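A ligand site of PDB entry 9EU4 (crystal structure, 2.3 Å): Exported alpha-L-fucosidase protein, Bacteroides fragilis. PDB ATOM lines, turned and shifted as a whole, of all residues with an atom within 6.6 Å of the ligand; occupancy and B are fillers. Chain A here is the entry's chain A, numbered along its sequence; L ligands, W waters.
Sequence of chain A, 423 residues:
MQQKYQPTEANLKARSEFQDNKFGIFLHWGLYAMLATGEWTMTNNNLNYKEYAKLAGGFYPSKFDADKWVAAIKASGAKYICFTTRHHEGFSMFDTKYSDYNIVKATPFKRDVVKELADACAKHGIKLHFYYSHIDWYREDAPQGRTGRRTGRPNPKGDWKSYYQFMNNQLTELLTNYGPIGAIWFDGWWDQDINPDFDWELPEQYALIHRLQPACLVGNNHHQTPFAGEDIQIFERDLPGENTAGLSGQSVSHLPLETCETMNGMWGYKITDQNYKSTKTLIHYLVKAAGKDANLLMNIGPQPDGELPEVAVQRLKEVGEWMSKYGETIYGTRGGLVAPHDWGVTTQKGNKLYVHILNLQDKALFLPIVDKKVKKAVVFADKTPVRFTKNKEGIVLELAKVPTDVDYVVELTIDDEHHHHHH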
ATOM      1  N   PHE A  26      34.936 -16.917 -18.138  1.00  0.00           N
ATOM      2  CA  PHE A  26      33.784 -17.496 -17.453  1.00  0.00           C
ATOM      3  C   PHE A  26      33.217 -16.511 -16.424  1.00  0.00           C
ATOM      4  O   PHE A  26      33.965 -16.026 -15.553  1.00  0.00           O
ATOM      5  CB  PHE A  26      34.188 -18.785 -16.718  1.00  0.00           C
ATOM      6  CG  PHE A  26      33.252 -19.956 -16.888  1.00  0.00           C
ATOM      7  CD1 PHE A  26      33.748 -21.270 -16.857  1.00  0.00           C
ATOM      8  CD2 PHE A  26      31.912 -19.775 -17.135  1.00  0.00           C
ATOM      9  CE1 PHE A  26      32.878 -22.359 -17.016  1.00  0.00           C
ATOM     10  CE2 PHE A  26      31.065 -20.859 -17.315  1.00  0.00           C
ATOM     11  CZ  PHE A  26      31.549 -22.142 -17.257  1.00  0.00           C
ATOM     12  N   HIS A  28      30.446 -16.536 -13.447  1.00  0.00           N
ATOM     13  CA  HIS A  28      29.528 -17.257 -12.552  1.00  0.00           C
ATOM     14  C   HIS A  28      28.841 -16.260 -11.631  1.00  0.00           C
ATOM     15  O   HIS A  28      29.444 -15.796 -10.657  1.00  0.00           O
ATOM     16  CB  HIS A  28      30.267 -18.299 -11.703  1.00  0.00           C
ATOM     17  CG  HIS A  28      30.399 -19.635 -12.354  1.00  0.00           C
ATOM     18  ND1 HIS A  28      31.382 -19.917 -13.273  1.00  0.00           N
ATOM     19  CD2 HIS A  28      29.675 -20.767 -12.214  1.00  0.00           C
ATOM     20  CE1 HIS A  28      31.258 -21.167 -13.681  1.00  0.00           C
ATOM     21  NE2 HIS A  28      30.229 -21.701 -13.050  1.00  0.00           N
ATOM     22  N   GLU A  39      28.697 -20.931  -5.216  1.00  0.00           N
ATOM     23  CA  GLU A  39      27.459 -21.288  -5.904  1.00  0.00           C
ATOM     24  C   GLU A  39      26.905 -22.641  -5.455  1.00  0.00           C
ATOM     25  O   GLU A  39      25.726 -22.925  -5.701  1.00  0.00           O
ATOM     26  CB  GLU A  39      27.694 -21.226  -7.433  1.00  0.00           C
ATOM     27  CG  GLU A  39      28.455 -22.437  -8.003  1.00  0.00           C
ATOM     28  CD  GLU A  39      29.957 -22.413  -7.691  1.00  0.00           C
ATOM     29  OE1 GLU A  39      30.428 -21.428  -7.053  1.00  0.00           O
ATOM     30  OE2 GLU A  39      30.640 -23.413  -7.999  1.00  0.00           O
ATOM     31  N   TRP A  40      27.693 -23.466  -4.764  1.00  0.00           N
ATOM     32  CA  TRP A  40      27.205 -24.718  -4.178  1.00  0.00           C
ATOM     33  C   TRP A  40      26.605 -24.557  -2.777  1.00  0.00           C
ATOM     34  O   TRP A  40      26.256 -25.564  -2.151  1.00  0.00           O
ATOM     35  CB  TRP A  40      28.338 -25.763  -4.146  1.00  0.00           C
ATOM     36  CG  TRP A  40      28.457 -26.461  -5.451  1.00  0.00           C
ATOM     37  CD1 TRP A  40      28.758 -25.888  -6.662  1.00  0.00           C
ATOM     38  CD2 TRP A  40      28.224 -27.843  -5.728  1.00  0.00           C
ATOM     39  NE1 TRP A  40      28.723 -26.820  -7.656  1.00  0.00           N
ATOM     40  CE2 TRP A  40      28.406 -28.037  -7.115  1.00  0.00           C
ATOM     41  CE3 TRP A  40      27.897 -28.944  -4.933  1.00  0.00           C
ATOM     42  CZ2 TRP A  40      28.254 -29.278  -7.735  1.00  0.00           C
ATOM     43  CZ3 TRP A  40      27.759 -30.186  -5.551  1.00  0.00           C
ATOM     44  CH2 TRP A  40      27.931 -30.338  -6.939  1.00  0.00           C
ATOM     45  N   THR A  84      26.717 -17.549 -16.891  1.00  0.00           N
ATOM     46  CA  THR A  84      25.758 -18.483 -16.293  1.00  0.00           C
ATOM     47  C   THR A  84      24.344 -17.924 -16.381  1.00  0.00           C
ATOM     48  O   THR A  84      23.939 -17.119 -15.535  1.00  0.00           O
ATOM     49  CB  THR A  84      26.118 -18.740 -14.826  1.00  0.00           C
ATOM     50  OG1 THR A  84      26.231 -17.486 -14.132  1.00  0.00           O
ATOM     51  CG2 THR A  84      27.407 -19.542 -14.665  1.00  0.00           C
ATOM     52  N   HIS A  87      22.095 -21.365 -12.952  1.00  0.00           N
ATOM     53  CA  HIS A  87      22.992 -22.374 -12.408  1.00  0.00           C
ATOM     54  C   HIS A  87      22.156 -23.368 -11.609  1.00  0.00           C
ATOM     55  O   HIS A  87      20.931 -23.428 -11.740  1.00  0.00           O
ATOM     56  CB  HIS A  87      24.096 -21.685 -11.596  1.00  0.00           C
ATOM     57  CG  HIS A  87      25.344 -22.515 -11.418  1.00  0.00           C
ATOM     58  ND1 HIS A  87      25.543 -23.334 -10.324  1.00  0.00           N
ATOM     59  CD2 HIS A  87      26.474 -22.595 -12.151  1.00  0.00           C
ATOM     60  CE1 HIS A  87      26.724 -23.910 -10.409  1.00  0.00           C
ATOM     61  NE2 HIS A  87      27.323 -23.472 -11.510  1.00  0.00           N
ATOM     62  N   HIS A  88      22.809 -24.169 -10.762  1.00  0.00           N
ATOM     63  CA  HIS A  88      22.106 -25.221 -10.025  1.00  0.00           C
ATOM     64  C   HIS A  88      21.068 -24.648  -9.075  1.00  0.00           C
ATOM     65  O   HIS A  88      20.061 -25.314  -8.800  1.00  0.00           O
ATOM     66  CB  HIS A  88      23.081 -26.090  -9.226  1.00  0.00           C
ATOM     67  CG  HIS A  88      24.246 -26.591 -10.027  1.00  0.00           C
ATOM     68  ND1 HIS A  88      24.174 -26.800 -11.384  1.00  0.00           N
ATOM     69  CD2 HIS A  88      25.504 -26.915  -9.655  1.00  0.00           C
ATOM     70  CE1 HIS A  88      25.343 -27.236 -11.818  1.00  0.00           C
ATOM     71  NE2 HIS A  88      26.174 -27.313 -10.797  1.00  0.00           N
ATOM     72  N   TYR A 131      25.967 -20.577 -20.243  1.00  0.00           N
ATOM     73  CA  TYR A 131      25.962 -21.737 -19.360  1.00  0.00           C
ATOM     74  C   TYR A 131      24.517 -22.058 -18.972  1.00  0.00           C
ATOM     75  O   TYR A 131      23.787 -21.146 -18.540  1.00  0.00           O
ATOM     76  CB  TYR A 131      26.821 -21.450 -18.127  1.00  0.00           C
ATOM     77  CG  TYR A 131      26.764 -22.509 -17.029  1.00  0.00           C
ATOM     78  CD1 TYR A 131      25.602 -22.696 -16.260  1.00  0.00           C
ATOM     79  CD2 TYR A 131      27.890 -23.288 -16.737  1.00  0.00           C
ATOM     80  CE1 TYR A 131      25.544 -23.648 -15.287  1.00  0.00           C
ATOM     81  CE2 TYR A 131      27.836 -24.256 -15.749  1.00  0.00           C
ATOM     82  CZ  TYR A 131      26.657 -24.424 -15.014  1.00  0.00           C
ATOM     83  OH  TYR A 131      26.575 -25.381 -14.020  1.00  0.00           O
ATOM     84  N   ILE A 135      20.515 -29.493 -13.941  1.00  0.00           N
ATOM     85  CA  ILE A 135      19.929 -29.835 -12.651  1.00  0.00           C
ATOM     86  C   ILE A 135      19.418 -28.568 -11.993  1.00  0.00           C
ATOM     87  O   ILE A 135      19.757 -27.449 -12.388  1.00  0.00           O
ATOM     88  CB  ILE A 135      20.920 -30.562 -11.725  1.00  0.00           C
ATOM     89  CG1 ILE A 135      21.999 -29.592 -11.250  1.00  0.00           C
ATOM     90  CG2 ILE A 135      21.519 -31.783 -12.451  1.00  0.00           C
ATOM     91  CD1 ILE A 135      23.112 -30.226 -10.401  1.00  0.00           C
ATOM     92  N   TRP A 185      26.483 -24.265 -23.176  1.00  0.00           N
ATOM     93  CA  TRP A 185      27.399 -24.990 -22.292  1.00  0.00           C
ATOM     94  C   TRP A 185      26.550 -25.699 -21.226  1.00  0.00           C
ATOM     95  O   TRP A 185      26.163 -25.081 -20.228  1.00  0.00           O
ATOM     96  CB  TRP A 185      28.348 -23.995 -21.648  1.00  0.00           C
ATOM     97  CG  TRP A 185      29.778 -24.365 -21.368  1.00  0.00           C
ATOM     98  CD1 TRP A 185      30.854 -24.150 -22.175  1.00  0.00           C
ATOM     99  CD2 TRP A 185      30.299 -24.921 -20.146  1.00  0.00           C
ATOM    100  NE1 TRP A 185      32.005 -24.578 -21.557  1.00  0.00           N
ATOM    101  CE2 TRP A 185      31.700 -25.048 -20.308  1.00  0.00           C
ATOM    102  CE3 TRP A 185      29.708 -25.350 -18.939  1.00  0.00           C
ATOM    103  CZ2 TRP A 185      32.523 -25.571 -19.298  1.00  0.00           C
ATOM    104  CZ3 TRP A 185      30.532 -25.878 -17.952  1.00  0.00           C
ATOM    105  CH2 TRP A 185      31.922 -25.984 -18.135  1.00  0.00           C
ATOM    106  N   ASP A 187      25.543 -28.267 -18.159  1.00  0.00           N
ATOM    107  CA  ASP A 187      26.237 -28.847 -17.008  1.00  0.00           C
ATOM    108  C   ASP A 187      25.239 -29.487 -16.050  1.00  0.00           C
ATOM    109  O   ASP A 187      24.085 -29.041 -15.946  1.00  0.00           O
ATOM    110  CB  ASP A 187      27.084 -27.779 -16.304  1.00  0.00           C
ATOM    111  CG  ASP A 187      27.822 -28.321 -15.110  1.00  0.00           C
ATOM    112  OD1 ASP A 187      28.558 -29.321 -15.261  1.00  0.00           O
ATOM    113  OD2 ASP A 187      27.667 -27.742 -14.012  1.00  0.00           O
ATOM    114  N   GLY A 188      25.687 -30.534 -15.354  1.00  0.00           N
ATOM    115  CA  GLY A 188      24.846 -31.235 -14.397  1.00  0.00           C
ATOM    116  C   GLY A 188      24.723 -32.738 -14.613  1.00  0.00           C
ATOM    117  O   GLY A 188      24.256 -33.453 -13.721  1.00  0.00           O
ATOM    118  N   TRP A 190      26.610 -35.247 -14.479  1.00  0.00           N
ATOM    119  CA  TRP A 190      27.190 -36.055 -13.417  1.00  0.00           C
ATOM    120  C   TRP A 190      26.245 -36.214 -12.211  1.00  0.00           C
ATOM    121  O   TRP A 190      26.431 -37.139 -11.426  1.00  0.00           O
ATOM    122  CB  TRP A 190      28.504 -35.419 -12.981  1.00  0.00           C
ATOM    123  CG  TRP A 190      28.456 -33.915 -12.990  1.00  0.00           C
ATOM    124  CD1 TRP A 190      28.955 -33.086 -13.945  1.00  0.00           C
ATOM    125  CD2 TRP A 190      27.853 -33.074 -11.997  1.00  0.00           C
ATOM    126  NE1 TRP A 190      28.721 -31.770 -13.615  1.00  0.00           N
ATOM    127  CE2 TRP A 190      28.040 -31.740 -12.420  1.00  0.00           C
ATOM    128  CE3 TRP A 190      27.191 -33.310 -10.785  1.00  0.00           C
ATOM    129  CZ2 TRP A 190      27.588 -30.659 -11.673  1.00  0.00           C
ATOM    130  CZ3 TRP A 190      26.732 -32.237 -10.057  1.00  0.00           C
ATOM    131  CH2 TRP A 190      26.932 -30.927 -10.501  1.00  0.00           C
ATOM    132  N   ASN A 221      29.439 -30.578 -19.952  1.00  0.00           N
ATOM    133  CA  ASN A 221      30.474 -30.867 -18.938  1.00  0.00           C
ATOM    134  C   ASN A 221      30.121 -32.147 -18.170  1.00  0.00           C
ATOM    135  O   ASN A 221      29.871 -32.152 -16.962  1.00  0.00           O
ATOM    136  CB  ASN A 221      30.627 -29.682 -17.999  1.00  0.00           C
ATOM    137  CG  ASN A 221      31.704 -29.915 -16.974  1.00  0.00           C
ATOM    138  OD1 ASN A 221      32.744 -30.524 -17.262  1.00  0.00           O
ATOM    139  ND2 ASN A 221      31.475 -29.421 -15.753  1.00  0.00           N
ATOM    140  N   HIS A 223      32.220 -34.951 -18.318  1.00  0.00           N
ATOM    141  CA  HIS A 223      33.442 -35.684 -17.994  1.00  0.00           C
ATOM    142  C   HIS A 223      33.486 -37.056 -18.675  1.00  0.00           C
ATOM    143  O   HIS A 223      34.148 -37.977 -18.195  1.00  0.00           O
ATOM    144  CB  HIS A 223      33.634 -35.833 -16.485  1.00  0.00           C
ATOM    145  CG  HIS A 223      33.561 -34.544 -15.731  1.00  0.00           C
ATOM    146  ND1 HIS A 223      32.919 -34.420 -14.519  1.00  0.00           N
ATOM    147  CD2 HIS A 223      34.069 -33.316 -16.003  1.00  0.00           C
ATOM    148  CE1 HIS A 223      33.026 -33.181 -14.085  1.00  0.00           C
ATOM    149  NE2 HIS A 223      33.718 -32.492 -14.962  1.00  0.00           N
ATOM    150  N   GLU A 236      37.497 -29.961 -17.202  1.00  0.00           N
ATOM    151  CA  GLU A 236      37.235 -29.109 -16.050  1.00  0.00           C
ATOM    152  C   GLU A 236      38.461 -29.099 -15.143  1.00  0.00           C
ATOM    153  O   GLU A 236      38.843 -30.135 -14.614  1.00  0.00           O
ATOM    154  CB  GLU A 236      36.004 -29.584 -15.281  1.00  0.00           C
ATOM    155  CG  GLU A 236      35.550 -28.627 -14.171  1.00  0.00           C
ATOM    156  CD  GLU A 236      34.451 -29.187 -13.292  1.00  0.00           C
ATOM    157  OE1 GLU A 236      33.760 -30.155 -13.688  1.00  0.00           O
ATOM    158  OE2 GLU A 236      34.256 -28.650 -12.191  1.00  0.00           O
ATOM    159  N   LEU A 247      38.919 -34.634 -11.959  1.00  0.00           N
ATOM    160  CA  LEU A 247      37.645 -34.572 -12.650  1.00  0.00           C
ATOM    161  C   LEU A 247      37.724 -34.966 -14.126  1.00  0.00           C
ATOM    162  O   LEU A 247      36.675 -34.969 -14.790  1.00  0.00           O
ATOM    163  CB  LEU A 247      37.021 -33.166 -12.538  1.00  0.00           C
ATOM    164  CG  LEU A 247      37.122 -32.347 -11.227  1.00  0.00           C
ATOM    165  CD1 LEU A 247      36.944 -30.848 -11.440  1.00  0.00           C
ATOM    166  CD2 LEU A 247      36.128 -32.846 -10.184  1.00  0.00           C
ATOM    167  N   CYS A 260      38.420 -25.289 -18.570  1.00  0.00           N
ATOM    168  CA  CYS A 260      37.960 -24.208 -17.707  1.00  0.00           C
ATOM    169  C   CYS A 260      38.711 -24.251 -16.383  1.00  0.00           C
ATOM    170  O   CYS A 260      39.206 -25.297 -15.952  1.00  0.00           O
ATOM    171  CB  CYS A 260      36.440 -24.253 -17.444  1.00  0.00           C
ATOM    172  SG  CYS A 260      35.726 -25.874 -16.981  1.00  0.00           S
ATOM    173  N   MET A 266      37.341 -20.367  -6.532  1.00  0.00           N
ATOM    174  CA  MET A 266      35.933 -20.704  -6.652  1.00  0.00           C
ATOM    175  C   MET A 266      35.331 -20.072  -7.904  1.00  0.00           C
ATOM    176  O   MET A 266      35.896 -19.144  -8.489  1.00  0.00           O
ATOM    177  CB  MET A 266      35.158 -20.280  -5.386  1.00  0.00           C
ATOM    178  CG  MET A 266      33.670 -20.670  -5.344  1.00  0.00           C
ATOM    179  SD  MET A 266      33.420 -22.466  -5.535  1.00  0.00           S
ATOM    180  CE  MET A 266      34.749 -23.150  -4.471  1.00  0.00           C
ATOM    181  N   TRP A 267      34.183 -20.612  -8.319  1.00  0.00           N
ATOM    182  CA  TRP A 267      33.497 -20.111  -9.503  1.00  0.00           C
ATOM    183  C   TRP A 267      32.660 -18.880  -9.152  1.00  0.00           C
ATOM    184  O   TRP A 267      32.897 -17.793  -9.682  1.00  0.00           O
ATOM    185  CB  TRP A 267      32.635 -21.209 -10.130  1.00  0.00           C
ATOM    186  CG  TRP A 267      33.447 -22.462 -10.457  1.00  0.00           C
ATOM    187  CD1 TRP A 267      33.511 -23.599  -9.717  1.00  0.00           C
ATOM    188  CD2 TRP A 267      34.295 -22.680 -11.595  1.00  0.00           C
ATOM    189  NE1 TRP A 267      34.351 -24.509 -10.303  1.00  0.00           N
ATOM    190  CE2 TRP A 267      34.837 -23.968 -11.463  1.00  0.00           C
ATOM    191  CE3 TRP A 267      34.640 -21.911 -12.711  1.00  0.00           C
ATOM    192  CZ2 TRP A 267      35.721 -24.509 -12.409  1.00  0.00           C
ATOM    193  CZ3 TRP A 267      35.517 -22.448 -13.645  1.00  0.00           C
ATOM    194  CH2 TRP A 267      36.037 -23.734 -13.485  1.00  0.00           C
HETATM  195  C1  LIG L   1      31.018 -27.897 -12.178  1.00  0.00           C
HETATM  196  C2  LIG L   1      29.895 -27.006 -11.658  1.00  0.00           C
HETATM  197  O1  LIG L   1      29.019 -27.645 -10.707  1.00  0.00           O
HETATM  198  C3  LIG L   1      30.589 -25.869 -11.003  1.00  0.00           C
HETATM  199  O2  LIG L   1      29.728 -25.194 -10.054  1.00  0.00           O
HETATM  200  C4  LIG L   1      31.042 -24.961 -12.097  1.00  0.00           C
HETATM  201  O3  LIG L   1      29.915 -24.523 -12.857  1.00  0.00           O
HETATM  202  C5  LIG L   1      32.005 -25.685 -13.044  1.00  0.00           C
HETATM  203  C6  LIG L   1      31.842 -25.071 -14.404  1.00  0.00           C
HETATM  204  O4  LIG L   1      31.839 -27.159 -13.201  1.00  0.00           O
HETATM  205  O5  LIG L   1      30.581 -29.052 -12.755  1.00  0.00           O
HETATM  206  O   HOH W   1      32.095 -31.442 -11.173  1.00  0.00           O
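Water W1 lies within hydrogen-bond range of O5 of the ligand and OE1 of Glu 236.
Merely in contact with the ligand: Phe 26 (3.9 Å), Tyr 131 (3.6 Å), Trp 185 (3.8 Å) and Trp 267 (3.7 Å). Hydrophobic or aromatic side chains within 4 Å of the ligand: Phe 26, His 28, Trp 40, His 87, His 88, Tyr 131, Trp 185, Trp 190 and Trp 267. Within 4 Å of the ligand: Phe 26, His 28, Glu 39, Trp 40, His 87, His 88, Tyr 131, Trp 185, Asp 187, Trp 190, Asn 221, Glu 236 and Trp 267. Along chain A the residues within 4 Å of the ligand span positions 26 to 267.
The side-chain amide nitrogen of Asn 221 sits at hydrogen-bond distance from the side-chain carboxylate of Glu 236 (3.2 Å). The side-chain carboxylate of Glu 236 sits at hydrogen-bond distance from a ring nitrogen (NE2) of His 223 (2.7 Å). A ring nitrogen (NE2) of His 87 is in hydrogen-bond range of the side-chain hydroxyl of Tyr 131 (3.2 Å). ND2 of Asn 221 lies within hydrogen-bond range of OD1 of Asp 187 (3.0 Å). NE2 of His 223 sits at hydrogen-bond distance from OD1 of Asn 221 (3.2 Å). The indole nitrogen (NE1) of Trp 190 lies within hydrogen-bond range of the side-chain carboxylate (OD1) of Asp 187. The side-chain carboxylate (OD2) of Asp 187 sits at hydrogen-bond distance from the side-chain hydroxyl (OH) of Tyr 131.
A ring nitrogen (NE2) of His 28 lies within hydrogen-bond range of an oxygen (O3) of the ligand, 2.8 Å away. A ring nitrogen (NE2) of His 88 is in hydrogen-bond range of an oxygen (O1) of the ligand, at 2.9 Å. OE2 of Glu 39 is in hydrogen-bond range of O2 of the ligand. The side-chain carboxylate (OE1) of Glu 236 sits at hydrogen-bond distance from an oxygen (O5) of the ligand, at 3.5 Å. NE1 of Trp 40 lies within hydrogen-bond range of O2 of the ligand. A ring nitrogen (NE2) of His 87 sits at hydrogen-bond distance from an oxygen (O3) of the ligand, at 3.1 Å. The side-chain amide nitrogen (ND2) of Asn 221 is in hydrogen-bond range of an oxygen (O5) of the ligand (3.2 Å). O5 of the ligand lies within hydrogen-bond range of OD1 of Asp 187. NE1 of Trp 190 lies within hydrogen-bond range of O5 of the ligand (3.4 Å).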
